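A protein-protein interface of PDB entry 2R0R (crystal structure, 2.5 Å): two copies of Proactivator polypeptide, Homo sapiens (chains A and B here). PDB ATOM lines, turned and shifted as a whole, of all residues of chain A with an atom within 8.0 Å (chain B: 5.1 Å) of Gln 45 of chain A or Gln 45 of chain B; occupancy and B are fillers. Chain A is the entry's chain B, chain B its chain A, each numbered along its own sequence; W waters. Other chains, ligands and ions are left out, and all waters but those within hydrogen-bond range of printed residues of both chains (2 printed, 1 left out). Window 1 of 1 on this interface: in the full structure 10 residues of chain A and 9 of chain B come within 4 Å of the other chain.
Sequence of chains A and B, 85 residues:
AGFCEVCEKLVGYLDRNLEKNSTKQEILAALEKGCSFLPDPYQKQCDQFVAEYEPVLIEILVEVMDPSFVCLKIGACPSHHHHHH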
ATOM      1  N   ALA A   1      -2.590  -4.009   5.229  1.00  0.00           N
ATOM      2  CA  ALA A   1      -2.005  -2.630   5.258  1.00  0.00           C
ATOM      3  C   ALA A   1      -2.259  -1.870   6.578  1.00  0.00           C
ATOM      4  O   ALA A   1      -1.738  -0.761   6.776  1.00  0.00           O
ATOM      5  CB  ALA A   1      -2.515  -1.818   4.069  1.00  0.00           C
ATOM      6  N   GLY A   2      -3.056  -2.472   7.467  1.00  0.00           N
ATOM      7  CA  GLY A   2      -3.481  -1.841   8.718  1.00  0.00           C
ATOM      8  C   GLY A   2      -2.350  -1.591   9.695  1.00  0.00           C
ATOM      9  O   GLY A   2      -2.390  -0.623  10.452  1.00  0.00           O
ATOM     10  N   PHE A   3      -1.341  -2.461   9.680  1.00  0.00           N
ATOM     11  CA  PHE A   3      -0.153  -2.271  10.518  1.00  0.00           C
ATOM     12  C   PHE A   3       1.020  -1.661   9.759  1.00  0.00           C
ATOM     13  O   PHE A   3       2.084  -1.446  10.338  1.00  0.00           O
ATOM     14  CB  PHE A   3       0.299  -3.593  11.155  1.00  0.00           C
ATOM     15  CG  PHE A   3      -0.525  -4.019  12.335  1.00  0.00           C
ATOM     16  CD1 PHE A   3      -0.749  -3.149  13.401  1.00  0.00           C
ATOM     17  CD2 PHE A   3      -1.053  -5.303  12.399  1.00  0.00           C
ATOM     18  CE1 PHE A   3      -1.502  -3.545  14.494  1.00  0.00           C
ATOM     19  CE2 PHE A   3      -1.800  -5.709  13.498  1.00  0.00           C
ATOM     20  CZ  PHE A   3      -2.023  -4.824  14.545  1.00  0.00           C
ATOM     21  N   CYS A   4       0.824  -1.385   8.470  1.00  0.00           N
ATOM     22  CA  CYS A   4       1.912  -0.955   7.594  1.00  0.00           C
ATOM     23  C   CYS A   4       2.591   0.328   8.055  1.00  0.00           C
ATOM     24  O   CYS A   4       3.820   0.393   8.126  1.00  0.00           O
ATOM     25  CB  CYS A   4       1.427  -0.780   6.158  1.00  0.00           C
ATOM     26  SG  CYS A   4       2.734  -0.197   5.037  1.00  0.00           S
ATOM     27  N   GLU A   5       1.785   1.345   8.351  1.00  0.00           N
ATOM     28  CA  GLU A   5       2.288   2.663   8.727  1.00  0.00           C
ATOM     29  C   GLU A   5       3.125   2.591   9.997  1.00  0.00           C
ATOM     30  O   GLU A   5       4.228   3.131  10.046  1.00  0.00           O
ATOM     31  CB  GLU A   5       1.128   3.660   8.886  1.00  0.00           C
ATOM     32  CG  GLU A   5       1.526   4.979   9.537  1.00  0.00           C
ATOM     33  CD  GLU A   5       0.414   6.020   9.542  1.00  0.00           C
ATOM     34  OE1 GLU A   5      -0.616   5.829  10.233  1.00  0.00           O
ATOM     35  OE2 GLU A   5       0.595   7.060   8.868  1.00  0.00           O
ATOM     36  N   VAL A   6       2.591   1.914  11.011  1.00  0.00           N
ATOM     37  CA  VAL A   6       3.235   1.819  12.324  1.00  0.00           C
ATOM     38  C   VAL A   6       4.489   0.923  12.297  1.00  0.00           C
ATOM     39  O   VAL A   6       5.454   1.148  13.043  1.00  0.00           O
ATOM     40  CB  VAL A   6       2.204   1.396  13.434  1.00  0.00           C
ATOM     41  CG1 VAL A   6       1.796  -0.065  13.305  1.00  0.00           C
ATOM     42  CG2 VAL A   6       2.743   1.697  14.828  1.00  0.00           C
ATOM     43  N   CYS A   7       4.472  -0.078  11.424  1.00  0.00           N
ATOM     44  CA  CYS A   7       5.635  -0.920  11.207  1.00  0.00           C
ATOM     45  C   CYS A   7       6.824  -0.068  10.807  1.00  0.00           C
ATOM     46  O   CYS A   7       7.887  -0.147  11.421  1.00  0.00           O
ATOM     47  CB  CYS A   7       5.363  -1.949  10.109  1.00  0.00           C
ATOM     48  SG  CYS A   7       6.750  -3.058   9.873  1.00  0.00           S
ATOM     49  N   LEU A  10       8.163   2.309  13.520  1.00  0.00           N
ATOM     50  CA  LEU A  10       8.874   1.597  14.569  1.00  0.00           C
ATOM     51  C   LEU A  10      10.228   1.073  14.086  1.00  0.00           C
ATOM     52  O   LEU A  10      11.250   1.319  14.731  1.00  0.00           O
ATOM     53  CB  LEU A  10       8.023   0.460  15.141  1.00  0.00           C
ATOM     54  CG  LEU A  10       8.721  -0.430  16.170  1.00  0.00           C
ATOM     55  CD1 LEU A  10       8.967   0.306  17.483  1.00  0.00           C
ATOM     56  CD2 LEU A  10       7.907  -1.669  16.396  1.00  0.00           C
ATOM     57  N   CYS A  35       8.061   1.360  21.014  1.00  0.00           N
ATOM     58  CA  CYS A  35       6.733   1.972  20.879  1.00  0.00           C
ATOM     59  C   CYS A  35       6.565   3.216  21.737  1.00  0.00           C
ATOM     60  O   CYS A  35       5.889   4.156  21.331  1.00  0.00           O
ATOM     61  CB  CYS A  35       5.633   0.960  21.196  1.00  0.00           C
ATOM     62  SG  CYS A  35       5.609  -0.450  20.067  1.00  0.00           S
ATOM     63  N   LEU A  38       7.558   6.430  19.890  1.00  0.00           N
ATOM     64  CA  LEU A  38       6.784   6.886  18.743  1.00  0.00           C
ATOM     65  C   LEU A  38       5.780   7.931  19.232  1.00  0.00           C
ATOM     66  O   LEU A  38       5.519   8.008  20.434  1.00  0.00           O
ATOM     67  CB  LEU A  38       6.089   5.701  18.052  1.00  0.00           C
ATOM     68  CG  LEU A  38       6.848   4.955  16.945  1.00  0.00           C
ATOM     69  CD1 LEU A  38       8.269   4.552  17.347  1.00  0.00           C
ATOM     70  CD2 LEU A  38       6.067   3.739  16.475  1.00  0.00           C
ATOM     71  N   ASP A  40       2.562   9.679  20.525  1.00  0.00           N
ATOM     72  CA  ASP A  40       1.516   9.128  21.390  1.00  0.00           C
ATOM     73  C   ASP A  40       0.340   8.440  20.656  1.00  0.00           C
ATOM     74  O   ASP A  40      -0.072   7.357  21.069  1.00  0.00           O
ATOM     75  CB  ASP A  40       0.999  10.186  22.382  1.00  0.00           C
ATOM     76  CG  ASP A  40       1.936  10.389  23.585  1.00  0.00           C
ATOM     77  OD1 ASP A  40       2.971  11.082  23.448  1.00  0.00           O
ATOM     78  OD2 ASP A  40       1.621   9.871  24.681  1.00  0.00           O
ATOM     79  N   PRO A  41      -0.198   9.050  19.574  1.00  0.00           N
ATOM     80  CA  PRO A  41      -1.306   8.399  18.850  1.00  0.00           C
ATOM     81  C   PRO A  41      -1.034   6.967  18.338  1.00  0.00           C
ATOM     82  O   PRO A  41      -1.980   6.218  18.082  1.00  0.00           O
ATOM     83  CB  PRO A  41      -1.554   9.345  17.670  1.00  0.00           C
ATOM     84  CG  PRO A  41      -1.066  10.670  18.135  1.00  0.00           C
ATOM     85  CD  PRO A  41       0.134  10.360  18.975  1.00  0.00           C
ATOM     86  N   TYR A  42       0.240   6.597  18.210  1.00  0.00           N
ATOM     87  CA  TYR A  42       0.641   5.291  17.695  1.00  0.00           C
ATOM     88  C   TYR A  42       0.887   4.242  18.775  1.00  0.00           C
ATOM     89  O   TYR A  42       1.083   3.073  18.451  1.00  0.00           O
ATOM     90  CB  TYR A  42       1.924   5.424  16.876  1.00  0.00           C
ATOM     91  CG  TYR A  42       1.772   6.106  15.542  1.00  0.00           C
ATOM     92  CD1 TYR A  42       1.905   7.487  15.423  1.00  0.00           C
ATOM     93  CD2 TYR A  42       1.525   5.366  14.389  1.00  0.00           C
ATOM     94  CE1 TYR A  42       1.770   8.115  14.186  1.00  0.00           C
ATOM     95  CE2 TYR A  42       1.389   5.977  13.153  1.00  0.00           C
ATOM     96  CZ  TYR A  42       1.510   7.351  13.055  1.00  0.00           C
ATOM     97  OH  TYR A  42       1.382   7.959  11.823  1.00  0.00           O
ATOM     98  N   GLN A  43       0.883   4.640  20.049  1.00  0.00           N
ATOM     99  CA  GLN A  43       1.392   3.760  21.116  1.00  0.00           C
ATOM    100  C   GLN A  43       0.717   2.398  21.178  1.00  0.00           C
ATOM    101  O   GLN A  43       1.394   1.372  21.062  1.00  0.00           O
ATOM    102  CB  GLN A  43       1.352   4.413  22.506  1.00  0.00           C
ATOM    103  CG  GLN A  43       2.194   3.634  23.553  1.00  0.00           C
ATOM    104  CD  GLN A  43       1.550   3.567  24.940  1.00  0.00           C
ATOM    105  OE1 GLN A  43       1.259   4.597  25.560  1.00  0.00           O
ATOM    106  NE2 GLN A  43       1.336   2.343  25.435  1.00  0.00           N
ATOM    107  N   LYS A  44      -0.601   2.388  21.366  1.00  0.00           N
ATOM    108  CA  LYS A  44      -1.326   1.135  21.563  1.00  0.00           C
ATOM    109  C   LYS A  44      -1.362   0.265  20.305  1.00  0.00           C
ATOM    110  O   LYS A  44      -1.332  -0.968  20.399  1.00  0.00           O
ATOM    111  CB  LYS A  44      -2.741   1.382  22.116  1.00  0.00           C
ATOM    112  CG  LYS A  44      -2.791   1.933  23.544  1.00  0.00           C
ATOM    113  CD  LYS A  44      -2.011   1.058  24.495  1.00  0.00           C
ATOM    114  CE  LYS A  44      -2.096   1.549  25.920  1.00  0.00           C
ATOM    115  NZ  LYS A  44      -1.418   0.583  26.841  1.00  0.00           N
ATOM    116  N   GLN A  45      -1.405   0.908  19.138  1.00  0.00           N
ATOM    117  CA  GLN A  45      -1.294   0.198  17.865  1.00  0.00           C
ATOM    118  C   GLN A  45       0.089  -0.444  17.701  1.00  0.00           C
ATOM    119  O   GLN A  45       0.208  -1.571  17.204  1.00  0.00           O
ATOM    120  CB  GLN A  45      -1.585   1.132  16.688  1.00  0.00           C
ATOM    121  CG  GLN A  45      -1.513   0.446  15.325  1.00  0.00           C
ATOM    122  CD  GLN A  45      -1.641   1.405  14.160  1.00  0.00           C
ATOM    123  OE1 GLN A  45      -1.066   2.495  14.164  1.00  0.00           O
ATOM    124  NE2 GLN A  45      -2.388   0.997  13.143  1.00  0.00           N
ATOM    125  N   CYS A  46       1.123   0.276  18.119  1.00  0.00           N
ATOM    126  CA  CYS A  46       2.489  -0.226  18.040  1.00  0.00           C
ATOM    127  C   CYS A  46       2.655  -1.445  18.944  1.00  0.00           C
ATOM    128  O   CYS A  46       3.217  -2.464  18.522  1.00  0.00           O
ATOM    129  CB  CYS A  46       3.494   0.875  18.409  1.00  0.00           C
ATOM    130  SG  CYS A  46       5.233   0.407  18.266  1.00  0.00           S
ATOM    131  N   ASP A  47       2.146  -1.340  20.172  1.00  0.00           N
ATOM    132  CA  ASP A  47       2.182  -2.432  21.140  1.00  0.00           C
ATOM    133  C   ASP A  47       1.559  -3.691  20.548  1.00  0.00           C
ATOM    134  O   ASP A  47       2.090  -4.789  20.703  1.00  0.00           O
ATOM    135  CB  ASP A  47       1.432  -2.041  22.419  1.00  0.00           C
ATOM    136  CG  ASP A  47       2.140  -0.950  23.220  1.00  0.00           C
ATOM    137  OD1 ASP A  47       3.343  -0.666  22.965  1.00  0.00           O
ATOM    138  OD2 ASP A  47       1.477  -0.380  24.125  1.00  0.00           O
ATOM    139  N   GLN A  48       0.433  -3.513  19.863  1.00  0.00           N
ATOM    140  CA  GLN A  48      -0.263  -4.610  19.217  1.00  0.00           C
ATOM    141  C   GLN A  48       0.542  -5.185  18.046  1.00  0.00           C
ATOM    142  O   GLN A  48       0.703  -6.397  17.949  1.00  0.00           O
ATOM    143  CB  GLN A  48      -1.649  -4.162  18.751  1.00  0.00           C
ATOM    144  CG  GLN A  48      -2.543  -5.304  18.291  1.00  0.00           C
ATOM    145  CD  GLN A  48      -3.873  -4.830  17.727  1.00  0.00           C
ATOM    146  OE1 GLN A  48      -4.144  -3.624  17.652  1.00  0.00           O
ATOM    147  NE2 GLN A  48      -4.717  -5.780  17.322  1.00  0.00           N
ATOM    148  N   PHE A  49       1.038  -4.313  17.166  1.00  0.00           N
ATOM    149  CA  PHE A  49       1.883  -4.731  16.053  1.00  0.00           C
ATOM    150  C   PHE A  49       3.074  -5.548  16.541  1.00  0.00           C
ATOM    151  O   PHE A  49       3.326  -6.646  16.043  1.00  0.00           O
ATOM    152  CB  PHE A  49       2.365  -3.526  15.239  1.00  0.00           C
ATOM    153  CG  PHE A  49       3.521  -3.842  14.320  1.00  0.00           C
ATOM    154  CD1 PHE A  49       3.339  -4.662  13.199  1.00  0.00           C
ATOM    155  CD2 PHE A  49       4.793  -3.333  14.579  1.00  0.00           C
ATOM    156  CE1 PHE A  49       4.405  -4.967  12.357  1.00  0.00           C
ATOM    157  CE2 PHE A  49       5.864  -3.636  13.744  1.00  0.00           C
ATOM    158  CZ  PHE A  49       5.669  -4.457  12.636  1.00  0.00           C
ATOM    159  N   VAL A  50       3.795  -5.010  17.520  1.00  0.00           N
ATOM    160  CA  VAL A  50       4.955  -5.697  18.094  1.00  0.00           C
ATOM    161  C   VAL A  50       4.593  -7.075  18.668  1.00  0.00           C
ATOM    162  O   VAL A  50       5.208  -8.077  18.303  1.00  0.00           O
ATOM    163  CB  VAL A  50       5.657  -4.831  19.161  1.00  0.00           C
ATOM    164  CG1 VAL A  50       6.743  -5.630  19.917  1.00  0.00           C
ATOM    165  CG2 VAL A  50       6.246  -3.613  18.517  1.00  0.00           C
ATOM    166  N   ALA A  51       3.597  -7.128  19.550  1.00  0.00           N
ATOM    167  CA  ALA A  51       3.137  -8.402  20.101  1.00  0.00           C
ATOM    168  C   ALA A  51       2.835  -9.420  19.000  1.00  0.00           C
ATOM    169  O   ALA A  51       3.170 -10.596  19.121  1.00  0.00           O
ATOM    170  CB  ALA A  51       1.905  -8.191  20.985  1.00  0.00           C
ATOM    171  N   GLU A  52       2.226  -8.953  17.919  1.00  0.00           N
ATOM    172  CA  GLU A  52       1.779  -9.837  16.866  1.00  0.00           C
ATOM    173  C   GLU A  52       2.913 -10.339  15.974  1.00  0.00           C
ATOM    174  O   GLU A  52       2.870 -11.474  15.503  1.00  0.00           O
ATOM    175  CB  GLU A  52       0.705  -9.144  16.033  1.00  0.00           C
ATOM    176  CG  GLU A  52      -0.334 -10.089  15.479  1.00  0.00           C
ATOM    177  CD  GLU A  52      -1.350  -9.393  14.600  1.00  0.00           C
ATOM    178  OE1 GLU A  52      -2.107  -8.541  15.111  1.00  0.00           O
ATOM    179  OE2 GLU A  52      -1.394  -9.717  13.395  1.00  0.00           O
ATOM    180  N   GLY B   2      -5.095  -7.834  21.339  1.00  0.00           N
ATOM    181  CA  GLY B   2      -5.768  -7.519  20.050  1.00  0.00           C
ATOM    182  C   GLY B   2      -6.525  -6.215  20.168  1.00  0.00           C
ATOM    183  O   GLY B   2      -6.018  -5.249  20.740  1.00  0.00           O
ATOM    184  N   PHE B   3      -7.752  -6.201  19.653  1.00  0.00           N
ATOM    185  CA  PHE B   3      -8.585  -5.005  19.648  1.00  0.00           C
ATOM    186  C   PHE B   3      -9.576  -4.931  20.815  1.00  0.00           C
ATOM    187  O   PHE B   3     -10.425  -4.036  20.850  1.00  0.00           O
ATOM    188  CB  PHE B   3      -9.366  -4.907  18.333  1.00  0.00           C
ATOM    189  CG  PHE B   3      -8.509  -4.703  17.118  1.00  0.00           C
ATOM    190  CD1 PHE B   3      -7.701  -3.577  16.991  1.00  0.00           C
ATOM    191  CD2 PHE B   3      -8.537  -5.629  16.073  1.00  0.00           C
ATOM    192  CE1 PHE B   3      -6.921  -3.392  15.848  1.00  0.00           C
ATOM    193  CE2 PHE B   3      -7.761  -5.448  14.928  1.00  0.00           C
ATOM    194  CZ  PHE B   3      -6.954  -4.330  14.818  1.00  0.00           C
ATOM    195  N   VAL B   6      -9.638  -1.513  23.152  1.00  0.00           N
ATOM    196  CA  VAL B   6     -10.029  -0.345  22.358  1.00  0.00           C
ATOM    197  C   VAL B   6     -11.499  -0.448  21.927  1.00  0.00           C
ATOM    198  O   VAL B   6     -12.223   0.547  21.912  1.00  0.00           O
ATOM    199  CB  VAL B   6      -9.061  -0.090  21.145  1.00  0.00           C
ATOM    200  CG1 VAL B   6      -9.189  -1.171  20.058  1.00  0.00           C
ATOM    201  CG2 VAL B   6      -9.277   1.294  20.561  1.00  0.00           C
ATOM    202  N   PRO B  41      -3.202   7.742  23.215  1.00  0.00           N
ATOM    203  CA  PRO B  41      -2.460   6.528  22.860  1.00  0.00           C
ATOM    204  C   PRO B  41      -3.293   5.481  22.118  1.00  0.00           C
ATOM    205  O   PRO B  41      -2.745   4.506  21.584  1.00  0.00           O
ATOM    206  CB  PRO B  41      -2.008   5.975  24.218  1.00  0.00           C
ATOM    207  CG  PRO B  41      -2.098   7.119  25.156  1.00  0.00           C
ATOM    208  CD  PRO B  41      -3.252   7.930  24.676  1.00  0.00           C
ATOM    209  N   TYR B  42      -4.604   5.700  22.066  1.00  0.00           N
ATOM    210  CA  TYR B  42      -5.509   4.754  21.450  1.00  0.00           C
ATOM    211  C   TYR B  42      -5.871   5.123  20.032  1.00  0.00           C
ATOM    212  O   TYR B  42      -6.391   4.294  19.297  1.00  0.00           O
ATOM    213  CB  TYR B  42      -6.773   4.627  22.289  1.00  0.00           C
ATOM    214  CG  TYR B  42      -6.569   3.834  23.552  1.00  0.00           C
ATOM    215  CD1 TYR B  42      -6.157   4.452  24.729  1.00  0.00           C
ATOM    216  CD2 TYR B  42      -6.786   2.460  23.567  1.00  0.00           C
ATOM    217  CE1 TYR B  42      -5.961   3.714  25.900  1.00  0.00           C
ATOM    218  CE2 TYR B  42      -6.596   1.714  24.720  1.00  0.00           C
ATOM    219  CZ  TYR B  42      -6.184   2.344  25.886  1.00  0.00           C
ATOM    220  OH  TYR B  42      -6.003   1.595  27.030  1.00  0.00           O
ATOM    221  N   GLN B  43      -5.585   6.357  19.637  1.00  0.00           N
ATOM    222  CA  GLN B  43      -6.220   6.925  18.444  1.00  0.00           C
ATOM    223  C   GLN B  43      -5.960   6.161  17.126  1.00  0.00           C
ATOM    224  O   GLN B  43      -6.895   5.942  16.351  1.00  0.00           O
ATOM    225  CB  GLN B  43      -5.985   8.450  18.353  1.00  0.00           C
ATOM    226  CG  GLN B  43      -4.996   8.948  17.313  1.00  0.00           C
ATOM    227  CD  GLN B  43      -5.651   9.386  15.997  1.00  0.00           C
ATOM    228  OE1 GLN B  43      -5.000  10.006  15.148  1.00  0.00           O
ATOM    229  NE2 GLN B  43      -6.938   9.062  15.822  1.00  0.00           N
ATOM    230  N   LYS B  44      -4.720   5.729  16.897  1.00  0.00           N
ATOM    231  CA  LYS B  44      -4.387   4.979  15.684  1.00  0.00           C
ATOM    232  C   LYS B  44      -4.926   3.549  15.710  1.00  0.00           C
ATOM    233  O   LYS B  44      -5.487   3.075  14.714  1.00  0.00           O
ATOM    234  CB  LYS B  44      -2.879   4.990  15.416  1.00  0.00           C
ATOM    235  CG  LYS B  44      -2.447   5.850  14.229  1.00  0.00           C
ATOM    236  CD  LYS B  44      -2.649   7.333  14.458  1.00  0.00           C
ATOM    237  CE  LYS B  44      -2.003   8.158  13.356  1.00  0.00           C
ATOM    238  NZ  LYS B  44      -2.857   8.255  12.135  1.00  0.00           N
ATOM    239  N   GLN B  45      -4.744   2.868  16.843  1.00  0.00           N
ATOM    240  CA  GLN B  45      -5.309   1.536  17.055  1.00  0.00           C
ATOM    241  C   GLN B  45      -6.809   1.568  16.814  1.00  0.00           C
ATOM    242  O   GLN B  45      -7.371   0.644  16.223  1.00  0.00           O
ATOM    243  CB  GLN B  45      -5.022   1.027  18.476  1.00  0.00           C
ATOM    244  CG  GLN B  45      -5.690  -0.319  18.805  1.00  0.00           C
ATOM    245  CD  GLN B  45      -5.213  -0.937  20.113  1.00  0.00           C
ATOM    246  OE1 GLN B  45      -5.176  -0.281  21.153  1.00  0.00           O
ATOM    247  NE2 GLN B  45      -4.859  -2.214  20.065  1.00  0.00           N
ATOM    248  N   CYS B  46      -7.445   2.640  17.272  1.00  0.00           N
ATOM    249  CA  CYS B  46      -8.882   2.781  17.178  1.00  0.00           C
ATOM    250  C   CYS B  46      -9.346   2.826  15.721  1.00  0.00           C
ATOM    251  O   CYS B  46     -10.240   2.073  15.325  1.00  0.00           O
ATOM    252  CB  CYS B  46      -9.340   4.027  17.937  1.00  0.00           C
ATOM    253  SG  CYS B  46     -11.125   4.209  18.009  1.00  0.00           S
ATOM    254  N   ASP B  47      -8.726   3.701  14.932  1.00  0.00           N
ATOM    255  CA  ASP B  47      -9.040   3.828  13.514  1.00  0.00           C
ATOM    256  C   ASP B  47      -8.904   2.485  12.793  1.00  0.00           C
ATOM    257  O   ASP B  47      -9.736   2.142  11.951  1.00  0.00           O
ATOM    258  CB  ASP B  47      -8.149   4.888  12.860  1.00  0.00           C
ATOM    259  CG  ASP B  47      -8.293   6.261  13.507  1.00  0.00           C
ATOM    260  OD1 ASP B  47      -9.373   6.557  14.061  1.00  0.00           O
ATOM    261  OD2 ASP B  47      -7.325   7.054  13.464  1.00  0.00           O
ATOM    262  N   GLN B  48      -7.862   1.729  13.132  1.00  0.00           N
ATOM    263  CA  GLN B  48      -7.650   0.408  12.547  1.00  0.00           C
ATOM    264  C   GLN B  48      -8.774  -0.552  12.914  1.00  0.00           C
ATOM    265  O   GLN B  48      -9.300  -1.244  12.053  1.00  0.00           O
ATOM    266  CB  GLN B  48      -6.301  -0.170  12.968  1.00  0.00           C
ATOM    267  CG  GLN B  48      -5.953  -1.471  12.269  1.00  0.00           C
ATOM    268  CD  GLN B  48      -4.643  -2.063  12.745  1.00  0.00           C
ATOM    269  OE1 GLN B  48      -3.916  -1.459  13.541  1.00  0.00           O
ATOM    270  NE2 GLN B  48      -4.327  -3.253  12.254  1.00  0.00           N
ATOM    271  N   PHE B  49      -9.135  -0.589  14.192  1.00  0.00           N
ATOM    272  CA  PHE B  49     -10.250  -1.410  14.658  1.00  0.00           C
ATOM    273  C   PHE B  49     -11.548  -1.105  13.892  1.00  0.00           C
ATOM    274  O   PHE B  49     -12.188  -2.012  13.347  1.00  0.00           O
ATOM    275  CB  PHE B  49     -10.445  -1.255  16.176  1.00  0.00           C
ATOM    276  CG  PHE B  49     -11.736  -1.840  16.681  1.00  0.00           C
ATOM    277  CD1 PHE B  49     -11.969  -3.213  16.612  1.00  0.00           C
ATOM    278  CD2 PHE B  49     -12.726  -1.015  17.217  1.00  0.00           C
ATOM    279  CE1 PHE B  49     -13.167  -3.753  17.061  1.00  0.00           C
ATOM    280  CE2 PHE B  49     -13.924  -1.541  17.669  1.00  0.00           C
ATOM    281  CZ  PHE B  49     -14.149  -2.912  17.586  1.00  0.00           C
HETATM  282  O   HOH W   1      -2.771  -1.968  22.316  1.00  0.00           O
HETATM  283  O   HOH W   2      -4.320   3.348  12.242  1.00  0.00           O
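Hydrophobic or aromatic side chains of chain A within 4 Å of the printed part of chain B: Phe 3, Pro 41 and Tyr 42.
Of the 12 printed residues of chain B, 8 touch a printed residue of chain A.
Among the printed residues, 18 pairs touch across the chains.
Among the printed residues, Asp or Glu carboxylates within 4 Å of a Lys or Arg side-chain nitrogen of the other chain: Glu 5 of chain A with Lys 44 of chain B (3.8 Å).
Gly 2 of chain A touches Gln 48 of chain B, and with the chains exchanged Gln 48 of chain A touches Gly 2 of chain B.
Pro 41 of chain A touches its own counterpart, Pro 41 of chain B.
Pro 41 of chain A touches Lys 44 of chain B, and with the chains exchanged Lys 44 of chain A touches Pro 41 of chain B.
Lys 44 of chain A touches Gln 45 of chain B, and with the chains exchanged Gln 45 of chain A touches Lys 44 of chain B.
Positions printed for both chains: 2, 3, 6, 41, 42, 43, 44, 45, 46, 47, 48 and 49.
Of the 18 pairs that touch across the chains among the printed residues, 16 have their exchanged pair printed and touching as well.
Among the printed residues, merely in contact across the chains: Asp 40 of chain A with Pro 41 of chain B, Lys 44 of chain A with Gln 45 of chain B, Gln 48 of chain A with Phe 3 of chain B, Gln 45 of chain A with Lys 44 of chain B, Phe 3 of chain A with Gln 48 of chain B, Gln 48 of chain A with Gly 2 of chain B, Pro 41 of chain A with Gln 43 of chain B, Gly 2 of chain A with Gln 48 of chain B, Gln 45 of chain A with Gln 45 of chain B, Tyr 42 of chain A with Lys 44 of chain B, Gln 43 of chain A with Pro 41 of chain B, Pro 41 of chain A with Pro 41 of chain B and Lys 44 of chain A with Tyr 42 of chain B.
O of Pro 41 of chain A lies within hydrogen-bond range of N of Lys 44 of chain B, at 3.0 Å.
The backbone NH (N) of Lys 44 of chain A lies within hydrogen-bond range of the backbone carbonyl oxygen (O) of Pro 41 of chain B, 3.0 Å away.
NE2 of Gln 45 of chain B lies within hydrogen-bond range of OE1 of Gln 48 of chain A, 2.9 Å away.
OE1 of Gln 48 of chain B sits at hydrogen-bond distance from NE2 of Gln 45 of chain A (2.9 Å).
OE1 of Glu 5 of chain A is in salt-bridge range of NZ of Lys 44 of chain B (3.8 Å).
NE2 of Gln 43 of chain A is in hydrogen-bond range of OD2 of Asp 47 of chain A.
O of Gly 2 of chain A sits at hydrogen-bond distance from NE2 of Gln 45 of chain A, 3.1 Å away.
OD2 of Asp 47 of chain B lies within hydrogen-bond range of NE2 of Gln 43 of chain B.
O of Gly 2 of chain B sits at hydrogen-bond distance from NE2 of Gln 45 of chain B.
SG of Cys 46 of chain A forms a disulfide with SG of Cys 35 of chain A.
The side-chain hydroxyl of Tyr 42 of chain A lies close to the side-chain carboxylate of Glu 5 of chain A, at 3.2 Å.
Water W1 bridges O of Lys 44 of chain A and NE2 of Gln 45 of chain B.
Water W2 bridges O of Lys 44 of chain B and NE2 of Gln 45 of chain A.
Of the printed residues of chain B, Glu 5 of chain A touches Lys 44.
Of the printed residues of chain B, Pro 41 of chain A touches Pro 41 (3.97 Å), Gln 43 (3.5 Å) and Lys 44 (3.0 Å).
Gln 45 of chain A touches three residues of chain B.
Printed residues of chain B within 4 Å of Gln 48 of chain A: Gly 2, Phe 3 and Gln 45.
Of the printed residues of chain A, Pro 41 of chain B touches Asp 40, Pro 41, Gln 43 and Lys 44.
Printed residues of chain A within 4 Å of Lys 44 of chain B: Glu 5, Pro 41, Tyr 42 and Gln 45.
Gln 45 of chain B touches three residues of chain A.
The nearest residue of chain A that does not touch Gln 45 of chain B is Pro 41 of chain A (4.5 Å).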
